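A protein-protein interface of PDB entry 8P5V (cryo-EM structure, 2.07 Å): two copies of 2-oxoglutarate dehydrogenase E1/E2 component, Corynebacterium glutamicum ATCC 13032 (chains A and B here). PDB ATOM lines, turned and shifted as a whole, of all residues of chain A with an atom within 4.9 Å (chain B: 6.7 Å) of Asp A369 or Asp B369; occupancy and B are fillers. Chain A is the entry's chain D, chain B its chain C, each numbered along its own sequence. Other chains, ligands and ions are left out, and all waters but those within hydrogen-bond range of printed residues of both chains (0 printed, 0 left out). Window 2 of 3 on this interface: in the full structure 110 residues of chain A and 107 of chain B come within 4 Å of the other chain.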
ATOM      1  N   ASN A 365      -0.098  35.245  -0.143  1.00  0.00           N
ATOM      2  CA  ASN A 365      -0.606  33.969   0.341  1.00  0.00           C
ATOM      3  C   ASN A 365      -1.099  34.152   1.772  1.00  0.00           C
ATOM      4  O   ASN A 365      -0.646  33.465   2.687  1.00  0.00           O
ATOM      5  CB  ASN A 365       0.445  32.861   0.218  1.00  0.00           C
ATOM      6  CG  ASN A 365      -0.103  31.469   0.465  1.00  0.00           C
ATOM      7  OD1 ASN A 365      -1.305  31.283   0.660  1.00  0.00           O
ATOM      8  ND2 ASN A 365       0.770  30.475   0.438  1.00  0.00           N
ATOM      9  N   GLY A 367      -4.621  34.756   4.459  1.00  0.00           N
ATOM     10  CA  GLY A 367      -5.959  34.216   4.614  1.00  0.00           C
ATOM     11  C   GLY A 367      -6.014  32.762   4.159  1.00  0.00           C
ATOM     12  O   GLY A 367      -5.187  31.954   4.576  1.00  0.00           O
ATOM     13  N   VAL A 368      -6.986  32.446   3.295  1.00  0.00           N
ATOM     14  CA  VAL A 368      -7.119  31.115   2.723  1.00  0.00           C
ATOM     15  C   VAL A 368      -5.853  30.787   1.931  1.00  0.00           C
ATOM     16  O   VAL A 368      -5.418  31.576   1.095  1.00  0.00           O
ATOM     17  CB  VAL A 368      -8.388  30.990   1.853  1.00  0.00           C
ATOM     18  CG1 VAL A 368      -8.526  32.124   0.844  1.00  0.00           C
ATOM     19  CG2 VAL A 368      -8.465  29.641   1.152  1.00  0.00           C
ATOM     20  N   ASP A 369      -5.265  29.619   2.217  1.00  0.00           N
ATOM     21  CA  ASP A 369      -4.023  29.202   1.585  1.00  0.00           C
ATOM     22  C   ASP A 369      -4.273  28.931   0.105  1.00  0.00           C
ATOM     23  O   ASP A 369      -5.363  28.514  -0.278  1.00  0.00           O
ATOM     24  CB  ASP A 369      -3.445  27.950   2.250  1.00  0.00           C
ATOM     25  CG  ASP A 369      -2.052  27.580   1.758  1.00  0.00           C
ATOM     26  OD1 ASP A 369      -1.380  28.450   1.158  1.00  0.00           O
ATOM     27  OD2 ASP A 369      -1.651  26.415   1.962  1.00  0.00           O
ATOM     28  N   LYS A 370      -3.241  29.153  -0.716  1.00  0.00           N
ATOM     29  CA  LYS A 370      -3.354  28.958  -2.148  1.00  0.00           C
ATOM     30  C   LYS A 370      -3.535  27.474  -2.473  1.00  0.00           C
ATOM     31  O   LYS A 370      -4.178  27.141  -3.462  1.00  0.00           O
ATOM     32  CB  LYS A 370      -2.150  29.582  -2.856  1.00  0.00           C
ATOM     33  CG  LYS A 370      -2.094  31.097  -2.776  1.00  0.00           C
ATOM     34  CD  LYS A 370      -1.166  31.736  -3.776  1.00  0.00           C
ATOM     35  CE  LYS A 370      -1.104  33.240  -3.624  1.00  0.00           C
ATOM     36  NZ  LYS A 370      -0.270  33.862  -4.682  1.00  0.00           N
ATOM     37  N   ASN A 371      -2.981  26.586  -1.642  1.00  0.00           N
ATOM     38  CA  ASN A 371      -3.218  25.160  -1.788  1.00  0.00           C
ATOM     39  C   ASN A 371      -4.712  24.864  -1.692  1.00  0.00           C
ATOM     40  O   ASN A 371      -5.224  24.009  -2.412  1.00  0.00           O
ATOM     41  CB  ASN A 371      -2.455  24.332  -0.751  1.00  0.00           C
ATOM     42  CG  ASN A 371      -1.002  24.102  -1.108  1.00  0.00           C
ATOM     43  OD1 ASN A 371      -0.556  24.433  -2.205  1.00  0.00           O
ATOM     44  ND2 ASN A 371      -0.252  23.526  -0.182  1.00  0.00           N
ATOM     45  N   THR A 372      -5.399  25.562  -0.783  1.00  0.00           N
ATOM     46  CA  THR A 372      -6.835  25.420  -0.633  1.00  0.00           C
ATOM     47  C   THR A 372      -7.536  25.852  -1.911  1.00  0.00           C
ATOM     48  O   THR A 372      -8.460  25.185  -2.375  1.00  0.00           O
ATOM     49  CB  THR A 372      -7.359  26.242   0.546  1.00  0.00           C
ATOM     50  OG1 THR A 372      -6.610  25.858   1.699  1.00  0.00           O
ATOM     51  CG2 THR A 372      -8.841  26.044   0.777  1.00  0.00           C
ATOM     52  N   ARG A 373      -7.077  26.977  -2.457  1.00  0.00           N
ATOM     53  CA  ARG A 373      -7.720  27.586  -3.598  1.00  0.00           C
ATOM     54  C   ARG A 373      -7.588  26.649  -4.796  1.00  0.00           C
ATOM     55  O   ARG A 373      -8.511  26.538  -5.597  1.00  0.00           O
ATOM     56  CB  ARG A 373      -7.104  28.964  -3.859  1.00  0.00           C
ATOM     57  CG  ARG A 373      -7.225  29.941  -2.694  1.00  0.00           C
ATOM     58  CD  ARG A 373      -6.381  31.191  -2.910  1.00  0.00           C
ATOM     59  NE  ARG A 373      -5.998  31.852  -1.669  1.00  0.00           N
ATOM     60  CZ  ARG A 373      -5.346  33.009  -1.596  1.00  0.00           C
ATOM     61  NH1 ARG A 373      -5.054  33.689  -2.688  1.00  0.00           N
ATOM     62  NH2 ARG A 373      -4.990  33.496  -0.425  1.00  0.00           N
ATOM     63  N   ASN B 365       0.867  17.734   8.632  1.00  0.00           N
ATOM     64  CA  ASN B 365       0.338  18.706   7.692  1.00  0.00           C
ATOM     65  C   ASN B 365       1.177  18.664   6.414  1.00  0.00           C
ATOM     66  O   ASN B 365       1.730  19.675   5.990  1.00  0.00           O
ATOM     67  CB  ASN B 365       0.296  20.106   8.317  1.00  0.00           C
ATOM     68  CG  ASN B 365      -0.494  21.106   7.498  1.00  0.00           C
ATOM     69  OD1 ASN B 365      -1.061  20.762   6.467  1.00  0.00           O
ATOM     70  ND2 ASN B 365      -0.524  22.353   7.941  1.00  0.00           N
ATOM     71  N   THR B 366       1.258  17.471   5.814  1.00  0.00           N
ATOM     72  CA  THR B 366       2.051  17.226   4.622  1.00  0.00           C
ATOM     73  C   THR B 366       1.100  16.880   3.481  1.00  0.00           C
ATOM     74  O   THR B 366      -0.031  16.455   3.707  1.00  0.00           O
ATOM     75  CB  THR B 366       3.073  16.104   4.858  1.00  0.00           C
ATOM     76  N   GLY B 367       1.583  17.050   2.246  1.00  0.00           N
ATOM     77  CA  GLY B 367       0.739  16.908   1.072  1.00  0.00           C
ATOM     78  C   GLY B 367      -0.296  18.027   1.016  1.00  0.00           C
ATOM     79  O   GLY B 367       0.049  19.199   1.150  1.00  0.00           O
ATOM     80  N   VAL B 368      -1.566  17.649   0.831  1.00  0.00           N
ATOM     81  CA  VAL B 368      -2.665  18.604   0.833  1.00  0.00           C
ATOM     82  C   VAL B 368      -2.726  19.283   2.201  1.00  0.00           C
ATOM     83  O   VAL B 368      -2.735  18.613   3.230  1.00  0.00           O
ATOM     84  CB  VAL B 368      -4.005  17.937   0.458  1.00  0.00           C
ATOM     85  CG1 VAL B 368      -4.277  16.670   1.262  1.00  0.00           C
ATOM     86  CG2 VAL B 368      -5.169  18.907   0.579  1.00  0.00           C
ATOM     87  N   ASP B 369      -2.754  20.621   2.197  1.00  0.00           N
ATOM     88  CA  ASP B 369      -2.752  21.403   3.423  1.00  0.00           C
ATOM     89  C   ASP B 369      -4.073  21.189   4.156  1.00  0.00           C
ATOM     90  O   ASP B 369      -5.105  20.964   3.531  1.00  0.00           O
ATOM     91  CB  ASP B 369      -2.554  22.892   3.132  1.00  0.00           C
ATOM     92  CG  ASP B 369      -2.390  23.768   4.362  1.00  0.00           C
ATOM     93  OD1 ASP B 369      -2.702  24.971   4.269  1.00  0.00           O
ATOM     94  OD2 ASP B 369      -1.933  23.246   5.402  1.00  0.00           O
ATOM     95  N   LYS B 370      -4.033  21.290   5.484  1.00  0.00           N
ATOM     96  CA  LYS B 370      -5.217  21.076   6.298  1.00  0.00           C
ATOM     97  C   LYS B 370      -6.228  22.200   6.075  1.00  0.00           C
ATOM     98  O   LYS B 370      -7.428  21.965   6.181  1.00  0.00           O
ATOM     99  CB  LYS B 370      -4.827  20.925   7.771  1.00  0.00           C
ATOM    100  CG  LYS B 370      -4.013  19.676   8.063  1.00  0.00           C
ATOM    101  CD  LYS B 370      -3.969  19.316   9.519  1.00  0.00           C
ATOM    102  CE  LYS B 370      -3.128  18.092   9.779  1.00  0.00           C
ATOM    103  NZ  LYS B 370      -3.249  17.648  11.178  1.00  0.00           N
ATOM    104  N   ASN B 371      -5.751  23.406   5.747  1.00  0.00           N
ATOM    105  CA  ASN B 371      -6.643  24.492   5.373  1.00  0.00           C
ATOM    106  C   ASN B 371      -7.476  24.085   4.161  1.00  0.00           C
ATOM    107  O   ASN B 371      -8.654  24.420   4.080  1.00  0.00           O
ATOM    108  CB  ASN B 371      -5.898  25.795   5.076  1.00  0.00           C
ATOM    109  CG  ASN B 371      -5.504  26.570   6.316  1.00  0.00           C
ATOM    110  OD1 ASN B 371      -5.921  26.242   7.423  1.00  0.00           O
ATOM    111  ND2 ASN B 371      -4.709  27.611   6.136  1.00  0.00           N
ATOM    112  N   THR B 372      -6.848  23.383   3.212  1.00  0.00           N
ATOM    113  CA  THR B 372      -7.543  22.884   2.041  1.00  0.00           C
ATOM    114  C   THR B 372      -8.622  21.898   2.456  1.00  0.00           C
ATOM    115  O   THR B 372      -9.738  21.943   1.945  1.00  0.00           O
ATOM    116  CB  THR B 372      -6.581  22.210   1.062  1.00  0.00           C
ATOM    117  OG1 THR B 372      -5.545  23.148   0.770  1.00  0.00           O
ATOM    118  CG2 THR B 372      -7.265  21.769  -0.210  1.00  0.00           C
ATOM    119  N   ARG B 373      -8.262  21.012   3.383  1.00  0.00           N
ATOM    120  CA  ARG B 373      -9.136  19.935   3.789  1.00  0.00           C
ATOM    121  C   ARG B 373     -10.367  20.526   4.466  1.00  0.00           C
ATOM    122  O   ARG B 373     -11.470  20.019   4.290  1.00  0.00           O
ATOM    123  CB  ARG B 373      -8.376  18.969   4.701  1.00  0.00           C
ATOM    124  CG  ARG B 373      -7.150  18.333   4.059  1.00  0.00           C
ATOM    125  CD  ARG B 373      -6.296  17.589   5.073  1.00  0.00           C
ATOM    126  NE  ARG B 373      -4.894  17.484   4.688  1.00  0.00           N
ATOM    127  CZ  ARG B 373      -3.974  16.788   5.352  1.00  0.00           C
ATOM    128  NH1 ARG B 373      -4.316  16.092   6.425  1.00  0.00           N
ATOM    129  NH2 ARG B 373      -2.712  16.803   4.938  1.00  0.00           N
ATOM    130  N   VAL B 374     -10.161  21.593   5.247  1.00  0.00           N
ATOM    131  CA  VAL B 374     -11.228  22.191   6.028  1.00  0.00           C
ATOM    132  C   VAL B 374     -12.255  22.798   5.080  1.00  0.00           C
ATOM    133  O   VAL B 374     -13.457  22.651   5.276  1.00  0.00           O
ATOM    134  CB  VAL B 374     -10.684  23.219   7.038  1.00  0.00           C
ATOM    135  CG1 VAL B 374     -11.764  24.150   7.553  1.00  0.00           C
ATOM    136  CG2 VAL B 374      -9.992  22.537   8.197  1.00  0.00           C
ATOM    137  N   HIS B 414     -11.578  13.545   4.868  1.00  0.00           N
ATOM    138  CA  HIS B 414     -10.828  14.720   4.458  1.00  0.00           C
ATOM    139  C   HIS B 414      -9.461  14.759   5.135  1.00  0.00           C
ATOM    140  O   HIS B 414      -8.818  15.808   5.144  1.00  0.00           O
ATOM    141  CB  HIS B 414     -11.634  15.983   4.775  1.00  0.00           C
ATOM    142  CG  HIS B 414     -12.975  16.006   4.122  1.00  0.00           C
ATOM    143  ND1 HIS B 414     -13.159  16.368   2.806  1.00  0.00           N
ATOM    144  CD2 HIS B 414     -14.185  15.718   4.603  1.00  0.00           C
ATOM    145  CE1 HIS B 414     -14.446  16.288   2.516  1.00  0.00           C
ATOM    146  NE2 HIS B 414     -15.085  15.895   3.591  1.00  0.00           N
ATOM    147  N   LEU B 416      -8.687  14.631   8.251  1.00  0.00           N
ATOM    148  CA  LEU B 416      -8.692  15.394   9.482  1.00  0.00           C
ATOM    149  C   LEU B 416      -9.019  14.439  10.626  1.00  0.00           C
ATOM    150  O   LEU B 416      -9.714  13.446  10.428  1.00  0.00           O
ATOM    151  CB  LEU B 416      -9.736  16.504   9.369  1.00  0.00           C
ATOM    152  CG  LEU B 416      -9.421  17.610   8.367  1.00  0.00           C
ATOM    153  CD1 LEU B 416     -10.628  18.492   8.129  1.00  0.00           C
ATOM    154  CD2 LEU B 416      -8.263  18.460   8.831  1.00  0.00           C
ATOM    155  N   PHE B 425      -7.865  27.369  11.550  1.00  0.00           N
ATOM    156  CA  PHE B 425      -7.720  27.296  10.110  1.00  0.00           C
ATOM    157  C   PHE B 425      -8.326  28.549   9.494  1.00  0.00           C
ATOM    158  O   PHE B 425      -9.224  29.148  10.076  1.00  0.00           O
ATOM    159  CB  PHE B 425      -8.389  26.028   9.573  1.00  0.00           C
ATOM    160  CG  PHE B 425      -7.861  24.752  10.176  1.00  0.00           C
ATOM    161  CD1 PHE B 425      -6.672  24.190   9.734  1.00  0.00           C
ATOM    162  CD2 PHE B 425      -8.528  24.143  11.222  1.00  0.00           C
ATOM    163  CE1 PHE B 425      -6.185  23.027  10.305  1.00  0.00           C
ATOM    164  CE2 PHE B 425      -8.031  22.988  11.796  1.00  0.00           C
ATOM    165  CZ  PHE B 425      -6.861  22.440  11.341  1.00  0.00           C
ATOM    166  N   ASN B 426      -7.829  28.922   8.314  1.00  0.00           N
ATOM    167  CA  ASN B 426      -8.369  30.036   7.553  1.00  0.00           C
ATOM    168  C   ASN B 426      -9.555  29.532   6.734  1.00  0.00           C
ATOM    169  O   ASN B 426      -9.400  28.633   5.908  1.00  0.00           O
ATOM    170  CB  ASN B 426      -7.324  30.673   6.633  1.00  0.00           C
ATOM    171  CG  ASN B 426      -6.054  31.073   7.350  1.00  0.00           C
ATOM    172  OD1 ASN B 426      -5.031  30.410   7.214  1.00  0.00           O
ATOM    173  ND2 ASN B 426      -6.125  32.128   8.144  1.00  0.00           N
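Among the printed residues, merely in contact across the chains: Val A368 with Asn B426.
OD2 of Asp B369 sits close to OD1 of Asn B365, 2.8 Å away. The side-chain amide oxygen (OD1) of Asn B426 is in hydrogen-bond range of the side-chain amide nitrogen (ND2) of Asn B371 (3.0 Å). OD1 of Asp A369 sits close to OD1 of Asn A365 (2.9 Å). The backbone carbonyl oxygen (O) of Val A368 is in hydrogen-bond range of the guanidinium group (NH2) of Arg A373.
Asp A369 touches one residue of chain B. Asp B369 touches one residue of chain A. Printed residues of chain B within 4 Å of Asn A371: Thr B372 (3.1 Å). Of the printed residues of chain B, Thr A372 touches Asn B371 (3.2 Å) and Thr B372 (2.9 Å). Of the printed residues of chain B, Gly A367 touches Asn B426 (3.0 Å). Of the printed residues of chain A, Asn B371 touches Thr A372. Of the printed residues of chain A, Thr B372 touches Asn A371 and Thr A372. Lys A370 touches none of the printed residues of chain B. The nearest residue of chain B that does not touch Asp A369 is Asn B371 (4.1 Å). The nearest residue of chain A that does not touch Asp B369 is Asn A371 (4.1 Å).
Asp A369 touches its own counterpart, Asp B369. Asn A371 touches Thr B372, and with the chains exchanged Thr A372 touches Asn B371. Thr B372 touches its own counterpart, Thr A372. 8 positions are printed for both chains.
O of Asn B371 sits close to OG1 of Thr A372 (3.5 Å). The backbone carbonyl oxygen (O) of Asn A371 lies close to the side-chain hydroxyl (OG1) of Thr B372 (3.3 Å). N of Thr A372 sits at hydrogen-bond distance from OG1 of Thr B372, 2.9 Å away. OD1 of Asn B426 sits close to O of Gly A367 (3.1 Å). The side-chain carboxylate (OD2) of Asp A369 lies close to the side-chain carboxylate (OD1) of Asp B369.
Of the 14 printed residues of chain B, 4 touch a printed residue of chain A. Printed residues of chain B that touch a printed residue of chain A: Asp B369, Asn B371, Thr B372 and Asn B426. Among the printed residues, 6 pairs touch across the chains. Among the printed residues, no Asp or Glu carboxylate lies within 4 Å of a Lys or Arg side-chain nitrogen of the other chain.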
